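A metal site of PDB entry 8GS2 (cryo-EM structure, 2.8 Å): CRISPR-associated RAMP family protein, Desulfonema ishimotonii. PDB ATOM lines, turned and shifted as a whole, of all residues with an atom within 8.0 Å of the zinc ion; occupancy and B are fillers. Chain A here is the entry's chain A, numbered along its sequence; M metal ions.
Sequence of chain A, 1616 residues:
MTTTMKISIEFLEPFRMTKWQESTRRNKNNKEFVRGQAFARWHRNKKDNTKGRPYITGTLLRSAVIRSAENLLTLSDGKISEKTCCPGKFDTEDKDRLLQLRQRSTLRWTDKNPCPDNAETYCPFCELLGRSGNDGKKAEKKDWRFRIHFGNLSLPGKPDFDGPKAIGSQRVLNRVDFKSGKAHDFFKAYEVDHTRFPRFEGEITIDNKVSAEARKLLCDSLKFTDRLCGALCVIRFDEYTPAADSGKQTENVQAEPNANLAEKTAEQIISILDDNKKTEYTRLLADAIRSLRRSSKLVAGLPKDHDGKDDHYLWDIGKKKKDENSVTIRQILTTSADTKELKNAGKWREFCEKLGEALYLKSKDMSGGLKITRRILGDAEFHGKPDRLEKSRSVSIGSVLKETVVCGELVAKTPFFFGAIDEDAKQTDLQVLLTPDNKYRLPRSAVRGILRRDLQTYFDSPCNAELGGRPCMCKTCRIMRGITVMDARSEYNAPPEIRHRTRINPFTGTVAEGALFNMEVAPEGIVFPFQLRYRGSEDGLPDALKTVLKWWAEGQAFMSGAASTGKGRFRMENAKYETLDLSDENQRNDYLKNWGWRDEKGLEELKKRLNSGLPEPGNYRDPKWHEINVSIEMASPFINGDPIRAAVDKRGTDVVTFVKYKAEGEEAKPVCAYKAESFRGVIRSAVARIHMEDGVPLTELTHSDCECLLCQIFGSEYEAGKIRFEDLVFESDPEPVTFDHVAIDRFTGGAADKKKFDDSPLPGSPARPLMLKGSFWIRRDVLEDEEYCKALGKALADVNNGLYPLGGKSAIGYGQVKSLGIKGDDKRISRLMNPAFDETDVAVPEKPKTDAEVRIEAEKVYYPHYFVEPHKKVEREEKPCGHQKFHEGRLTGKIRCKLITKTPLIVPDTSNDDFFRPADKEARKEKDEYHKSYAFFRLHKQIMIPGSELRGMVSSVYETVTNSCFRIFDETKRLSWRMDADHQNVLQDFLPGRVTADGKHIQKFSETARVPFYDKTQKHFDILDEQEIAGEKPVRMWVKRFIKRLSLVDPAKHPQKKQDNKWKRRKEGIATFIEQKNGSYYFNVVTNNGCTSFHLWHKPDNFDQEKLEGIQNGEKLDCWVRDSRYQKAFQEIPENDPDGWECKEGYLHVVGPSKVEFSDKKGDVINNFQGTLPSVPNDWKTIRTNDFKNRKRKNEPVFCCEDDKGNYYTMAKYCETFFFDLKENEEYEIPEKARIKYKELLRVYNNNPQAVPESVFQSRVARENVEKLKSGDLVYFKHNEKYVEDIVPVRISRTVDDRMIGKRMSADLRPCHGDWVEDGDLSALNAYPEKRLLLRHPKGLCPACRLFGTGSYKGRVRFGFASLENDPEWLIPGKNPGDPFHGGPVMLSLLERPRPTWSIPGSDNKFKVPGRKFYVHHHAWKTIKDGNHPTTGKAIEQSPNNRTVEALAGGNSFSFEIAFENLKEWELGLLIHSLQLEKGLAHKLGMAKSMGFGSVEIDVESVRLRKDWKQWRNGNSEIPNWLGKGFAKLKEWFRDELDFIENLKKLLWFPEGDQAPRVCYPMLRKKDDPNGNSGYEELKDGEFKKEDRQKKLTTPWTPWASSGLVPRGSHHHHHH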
ATOM      1  N   ARG A 684     -29.573 -17.590  -0.137  1.00  0.00           N
ATOM      2  CA  ARG A 684     -28.731 -16.683  -0.910  1.00  0.00           C
ATOM      3  C   ARG A 684     -29.385 -16.325  -2.245  1.00  0.00           C
ATOM      4  O   ARG A 684     -29.305 -15.169  -2.694  1.00  0.00           O
ATOM      5  CB  ARG A 684     -27.356 -17.309  -1.132  1.00  0.00           C
ATOM      6  CG  ARG A 684     -26.405 -16.466  -1.950  1.00  0.00           C
ATOM      7  CD  ARG A 684     -25.042 -17.117  -2.029  1.00  0.00           C
ATOM      8  NE  ARG A 684     -24.135 -16.386  -2.910  1.00  0.00           N
ATOM      9  CZ  ARG A 684     -24.026 -16.616  -4.212  1.00  0.00           C
ATOM     10  NH1 ARG A 684     -24.741 -17.537  -4.814  1.00  0.00           N
ATOM     11  NH2 ARG A 684     -23.164 -15.881  -4.914  1.00  0.00           N
ATOM     12  N   GLU A 693     -27.536  -3.897  -7.528  1.00  0.00           N
ATOM     13  CA  GLU A 693     -26.358  -3.093  -7.240  1.00  0.00           C
ATOM     14  C   GLU A 693     -26.140  -2.145  -8.417  1.00  0.00           C
ATOM     15  O   GLU A 693     -25.738  -2.582  -9.499  1.00  0.00           O
ATOM     16  CB  GLU A 693     -25.133  -3.965  -7.014  1.00  0.00           C
ATOM     17  CG  GLU A 693     -23.839  -3.203  -6.763  1.00  0.00           C
ATOM     18  CD  GLU A 693     -23.743  -2.654  -5.347  1.00  0.00           C
ATOM     19  OE1 GLU A 693     -24.661  -2.886  -4.544  1.00  0.00           O
ATOM     20  OE2 GLU A 693     -22.726  -1.981  -5.043  1.00  0.00           O
ATOM     21  N   PRO A 697     -28.873  -6.547 -11.132  1.00  0.00           N
ATOM     22  CA  PRO A 697     -29.210  -7.543 -10.115  1.00  0.00           C
ATOM     23  C   PRO A 697     -27.971  -8.202  -9.536  1.00  0.00           C
ATOM     24  O   PRO A 697     -26.946  -8.353 -10.212  1.00  0.00           O
ATOM     25  CB  PRO A 697     -30.072  -8.557 -10.885  1.00  0.00           C
ATOM     26  CG  PRO A 697     -30.610  -7.796 -12.048  1.00  0.00           C
ATOM     27  CD  PRO A 697     -29.537  -6.828 -12.424  1.00  0.00           C
ATOM     28  N   LEU A 698     -28.067  -8.593  -8.263  1.00  0.00           N
ATOM     29  CA  LEU A 698     -26.941  -9.238  -7.601  1.00  0.00           C
ATOM     30  C   LEU A 698     -26.620 -10.607  -8.194  1.00  0.00           C
ATOM     31  O   LEU A 698     -25.499 -11.097  -8.024  1.00  0.00           O
ATOM     32  CB  LEU A 698     -27.219  -9.389  -6.108  1.00  0.00           C
ATOM     33  CG  LEU A 698     -27.455  -8.107  -5.307  1.00  0.00           C
ATOM     34  CD1 LEU A 698     -27.579  -8.417  -3.833  1.00  0.00           C
ATOM     35  CD2 LEU A 698     -26.351  -7.108  -5.554  1.00  0.00           C
ATOM     36  N   LEU A 701     -23.877 -10.120 -11.108  1.00  0.00           N
ATOM     37  CA  LEU A 701     -22.585  -9.531 -10.812  1.00  0.00           C
ATOM     38  C   LEU A 701     -21.506 -10.607 -10.796  1.00  0.00           C
ATOM     39  O   LEU A 701     -21.744 -11.771 -10.475  1.00  0.00           O
ATOM     40  CB  LEU A 701     -22.609  -8.818  -9.468  1.00  0.00           C
ATOM     41  CG  LEU A 701     -23.621  -7.684  -9.301  1.00  0.00           C
ATOM     42  CD1 LEU A 701     -23.501  -7.083  -7.912  1.00  0.00           C
ATOM     43  CD2 LEU A 701     -23.426  -6.624 -10.361  1.00  0.00           C
ATOM     44  N   THR A 702     -20.283 -10.191 -11.157  1.00  0.00           N
ATOM     45  CA  THR A 702     -19.110 -11.058 -11.052  1.00  0.00           C
ATOM     46  C   THR A 702     -18.487 -11.028  -9.660  1.00  0.00           C
ATOM     47  O   THR A 702     -17.635 -11.872  -9.367  1.00  0.00           O
ATOM     48  CB  THR A 702     -18.065 -10.668 -12.094  1.00  0.00           C
ATOM     49  OG1 THR A 702     -17.688  -9.300 -11.909  1.00  0.00           O
ATOM     50  CG2 THR A 702     -18.619 -10.848 -13.499  1.00  0.00           C
ATOM     51  N   HIS A 703     -18.888 -10.077  -8.822  1.00  0.00           N
ATOM     52  CA  HIS A 703     -18.438  -9.984  -7.433  1.00  0.00           C
ATOM     53  C   HIS A 703     -16.912  -9.864  -7.333  1.00  0.00           C
ATOM     54  O   HIS A 703     -16.266 -10.471  -6.478  1.00  0.00           O
ATOM     55  CB  HIS A 703     -18.949 -11.161  -6.604  1.00  0.00           C
ATOM     56  CG  HIS A 703     -20.447 -11.201  -6.490  1.00  0.00           C
ATOM     57  ND1 HIS A 703     -21.162 -10.319  -5.713  1.00  0.00           N
ATOM     58  CD2 HIS A 703     -21.363 -12.018  -7.071  1.00  0.00           C
ATOM     59  CE1 HIS A 703     -22.448 -10.596  -5.816  1.00  0.00           C
ATOM     60  NE2 HIS A 703     -22.597 -11.619  -6.637  1.00  0.00           N
ATOM     61  N   SER A 704     -16.337  -9.076  -8.245  1.00  0.00           N
ATOM     62  CA  SER A 704     -14.917  -8.746  -8.213  1.00  0.00           C
ATOM     63  C   SER A 704     -14.800  -7.259  -7.925  1.00  0.00           C
ATOM     64  O   SER A 704     -15.407  -6.433  -8.624  1.00  0.00           O
ATOM     65  CB  SER A 704     -14.230  -9.093  -9.530  1.00  0.00           C
ATOM     66  OG  SER A 704     -14.764  -8.324 -10.599  1.00  0.00           O
ATOM     67  N   ASP A 705     -14.015  -6.899  -6.901  1.00  0.00           N
ATOM     68  CA  ASP A 705     -13.968  -5.534  -6.371  1.00  0.00           C
ATOM     69  C   ASP A 705     -15.359  -5.050  -5.997  1.00  0.00           C
ATOM     70  O   ASP A 705     -15.729  -3.901  -6.249  1.00  0.00           O
ATOM     71  CB  ASP A 705     -13.307  -4.570  -7.369  1.00  0.00           C
ATOM     72  CG  ASP A 705     -11.828  -4.838  -7.537  1.00  0.00           C
ATOM     73  OD1 ASP A 705     -11.145  -5.086  -6.517  1.00  0.00           O
ATOM     74  OD2 ASP A 705     -11.338  -4.805  -8.687  1.00  0.00           O
ATOM     75  N   CYS A 706     -16.144  -5.935  -5.389  1.00  0.00           N
ATOM     76  CA  CYS A 706     -17.551  -5.706  -5.122  1.00  0.00           C
ATOM     77  C   CYS A 706     -17.788  -5.542  -3.628  1.00  0.00           C
ATOM     78  O   CYS A 706     -17.118  -6.188  -2.809  1.00  0.00           O
ATOM     79  CB  CYS A 706     -18.403  -6.854  -5.663  1.00  0.00           C
ATOM     80  SG  CYS A 706     -20.175  -6.662  -5.452  1.00  0.00           S
ATOM     81  N   GLU A 707     -18.747  -4.682  -3.276  1.00  0.00           N
ATOM     82  CA  GLU A 707     -19.102  -4.438  -1.885  1.00  0.00           C
ATOM     83  C   GLU A 707     -20.625  -4.465  -1.701  1.00  0.00           C
ATOM     84  O   GLU A 707     -21.163  -3.778  -0.836  1.00  0.00           O
ATOM     85  CB  GLU A 707     -18.534  -3.107  -1.395  1.00  0.00           C
ATOM     86  CG  GLU A 707     -18.886  -1.925  -2.279  1.00  0.00           C
ATOM     87  CD  GLU A 707     -18.201  -0.647  -1.834  1.00  0.00           C
ATOM     88  OE1 GLU A 707     -17.307  -0.713  -0.962  1.00  0.00           O
ATOM     89  OE2 GLU A 707     -18.560   0.435  -2.354  1.00  0.00           O
ATOM     90  N   CYS A 708     -21.315  -5.263  -2.508  1.00  0.00           N
ATOM     91  CA  CYS A 708     -22.765  -5.389  -2.389  1.00  0.00           C
ATOM     92  C   CYS A 708     -23.123  -6.153  -1.119  1.00  0.00           C
ATOM     93  O   CYS A 708     -22.277  -6.774  -0.476  1.00  0.00           O
ATOM     94  CB  CYS A 708     -23.355  -6.074  -3.616  1.00  0.00           C
ATOM     95  SG  CYS A 708     -23.219  -7.872  -3.597  1.00  0.00           S
ATOM     96  N   LEU A 709     -24.409  -6.109  -0.754  1.00  0.00           N
ATOM     97  CA  LEU A 709     -24.842  -6.773   0.466  1.00  0.00           C
ATOM     98  C   LEU A 709     -24.747  -8.287   0.373  1.00  0.00           C
ATOM     99  O   LEU A 709     -24.620  -8.945   1.409  1.00  0.00           O
ATOM    100  CB  LEU A 709     -26.275  -6.346   0.811  1.00  0.00           C
ATOM    101  CG  LEU A 709     -27.398  -6.477  -0.207  1.00  0.00           C
ATOM    102  CD1 LEU A 709     -28.011  -7.865  -0.200  1.00  0.00           C
ATOM    103  CD2 LEU A 709     -28.464  -5.417   0.054  1.00  0.00           C
ATOM    104  N   LEU A 710     -24.781  -8.858  -0.831  1.00  0.00           N
ATOM    105  CA  LEU A 710     -24.590 -10.297  -0.952  1.00  0.00           C
ATOM    106  C   LEU A 710     -23.182 -10.692  -0.541  1.00  0.00           C
ATOM    107  O   LEU A 710     -22.993 -11.664   0.205  1.00  0.00           O
ATOM    108  CB  LEU A 710     -24.884 -10.744  -2.391  1.00  0.00           C
ATOM    109  CG  LEU A 710     -25.018 -12.252  -2.622  1.00  0.00           C
ATOM    110  CD1 LEU A 710     -26.241 -12.774  -1.899  1.00  0.00           C
ATOM    111  CD2 LEU A 710     -25.089 -12.564  -4.100  1.00  0.00           C
ATOM    112  N   CYS A 711     -22.174  -9.948  -1.005  1.00  0.00           N
ATOM    113  CA  CYS A 711     -20.794 -10.218  -0.597  1.00  0.00           C
ATOM    114  C   CYS A 711     -20.534  -9.844   0.846  1.00  0.00           C
ATOM    115  O   CYS A 711     -19.582 -10.361   1.449  1.00  0.00           O
ATOM    116  CB  CYS A 711     -19.819  -9.461  -1.507  1.00  0.00           C
ATOM    117  SG  CYS A 711     -19.953  -9.844  -3.265  1.00  0.00           S
ATOM    118  N   GLN A 712     -21.337  -8.946   1.423  1.00  0.00           N
ATOM    119  CA  GLN A 712     -21.133  -8.508   2.795  1.00  0.00           C
ATOM    120  C   GLN A 712     -21.897  -9.358   3.799  1.00  0.00           C
ATOM    121  O   GLN A 712     -21.612  -9.277   4.996  1.00  0.00           O
ATOM    122  CB  GLN A 712     -21.538  -7.045   2.944  1.00  0.00           C
ATOM    123  CG  GLN A 712     -20.578  -6.088   2.260  1.00  0.00           C
ATOM    124  CD  GLN A 712     -21.057  -4.648   2.295  1.00  0.00           C
ATOM    125  OE1 GLN A 712     -22.231  -4.386   2.524  1.00  0.00           O
ATOM    126  NE2 GLN A 712     -20.137  -3.715   2.068  1.00  0.00           N
ATOM    127  N   GLY A 715     -20.690 -13.518   1.897  1.00  0.00           N
ATOM    128  CA  GLY A 715     -19.291 -13.620   1.537  1.00  0.00           C
ATOM    129  C   GLY A 715     -19.094 -13.834   0.051  1.00  0.00           C
ATOM    130  O   GLY A 715     -20.029 -14.019  -0.721  1.00  0.00           O
ATOM    131  N   SER A 716     -17.825 -13.809  -0.347  1.00  0.00           N
ATOM    132  CA  SER A 716     -17.443 -14.020  -1.739  1.00  0.00           C
ATOM    133  C   SER A 716     -16.212 -14.910  -1.753  1.00  0.00           C
ATOM    134  O   SER A 716     -15.817 -15.469  -0.725  1.00  0.00           O
ATOM    135  CB  SER A 716     -17.194 -12.686  -2.445  1.00  0.00           C
ATOM    136  OG  SER A 716     -16.144 -11.962  -1.809  1.00  0.00           O
ATOM    137  N   GLU A 719     -13.460 -13.212   0.593  1.00  0.00           N
ATOM    138  CA  GLU A 719     -13.664 -12.956   2.013  1.00  0.00           C
ATOM    139  C   GLU A 719     -14.697 -13.927   2.563  1.00  0.00           C
ATOM    140  O   GLU A 719     -15.541 -14.438   1.819  1.00  0.00           O
ATOM    141  CB  GLU A 719     -14.114 -11.509   2.254  1.00  0.00           C
ATOM    142  CG  GLU A 719     -15.418 -11.150   1.578  1.00  0.00           C
ATOM    143  CD  GLU A 719     -15.830  -9.717   1.854  1.00  0.00           C
ATOM    144  OE1 GLU A 719     -15.180  -9.070   2.693  1.00  0.00           O
ATOM    145  OE2 GLU A 719     -16.802  -9.248   1.227  1.00  0.00           O
HETATM  146 ZN    ZN M   1     -21.268  -8.532  -4.658  1.00  0.00          ZN
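Four residues have an atom within 4 Å of the zinc ion: His 703, Cys 706, Cys 708 and Cys 711.
The zinc ion is bound by ND1 of His 703 (2.1 Å), SG of Cys 706 (2.3 Å), SG of Cys 708 (2.3 Å) and SG of Cys 711 (2.3 Å).
A ring nitrogen (NE2) of His 703 lies within hydrogen-bond range of the backbone carbonyl oxygen (O) of Leu 698 (3.3 Å). N of Leu 710 sits close to SG of Cys 708.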
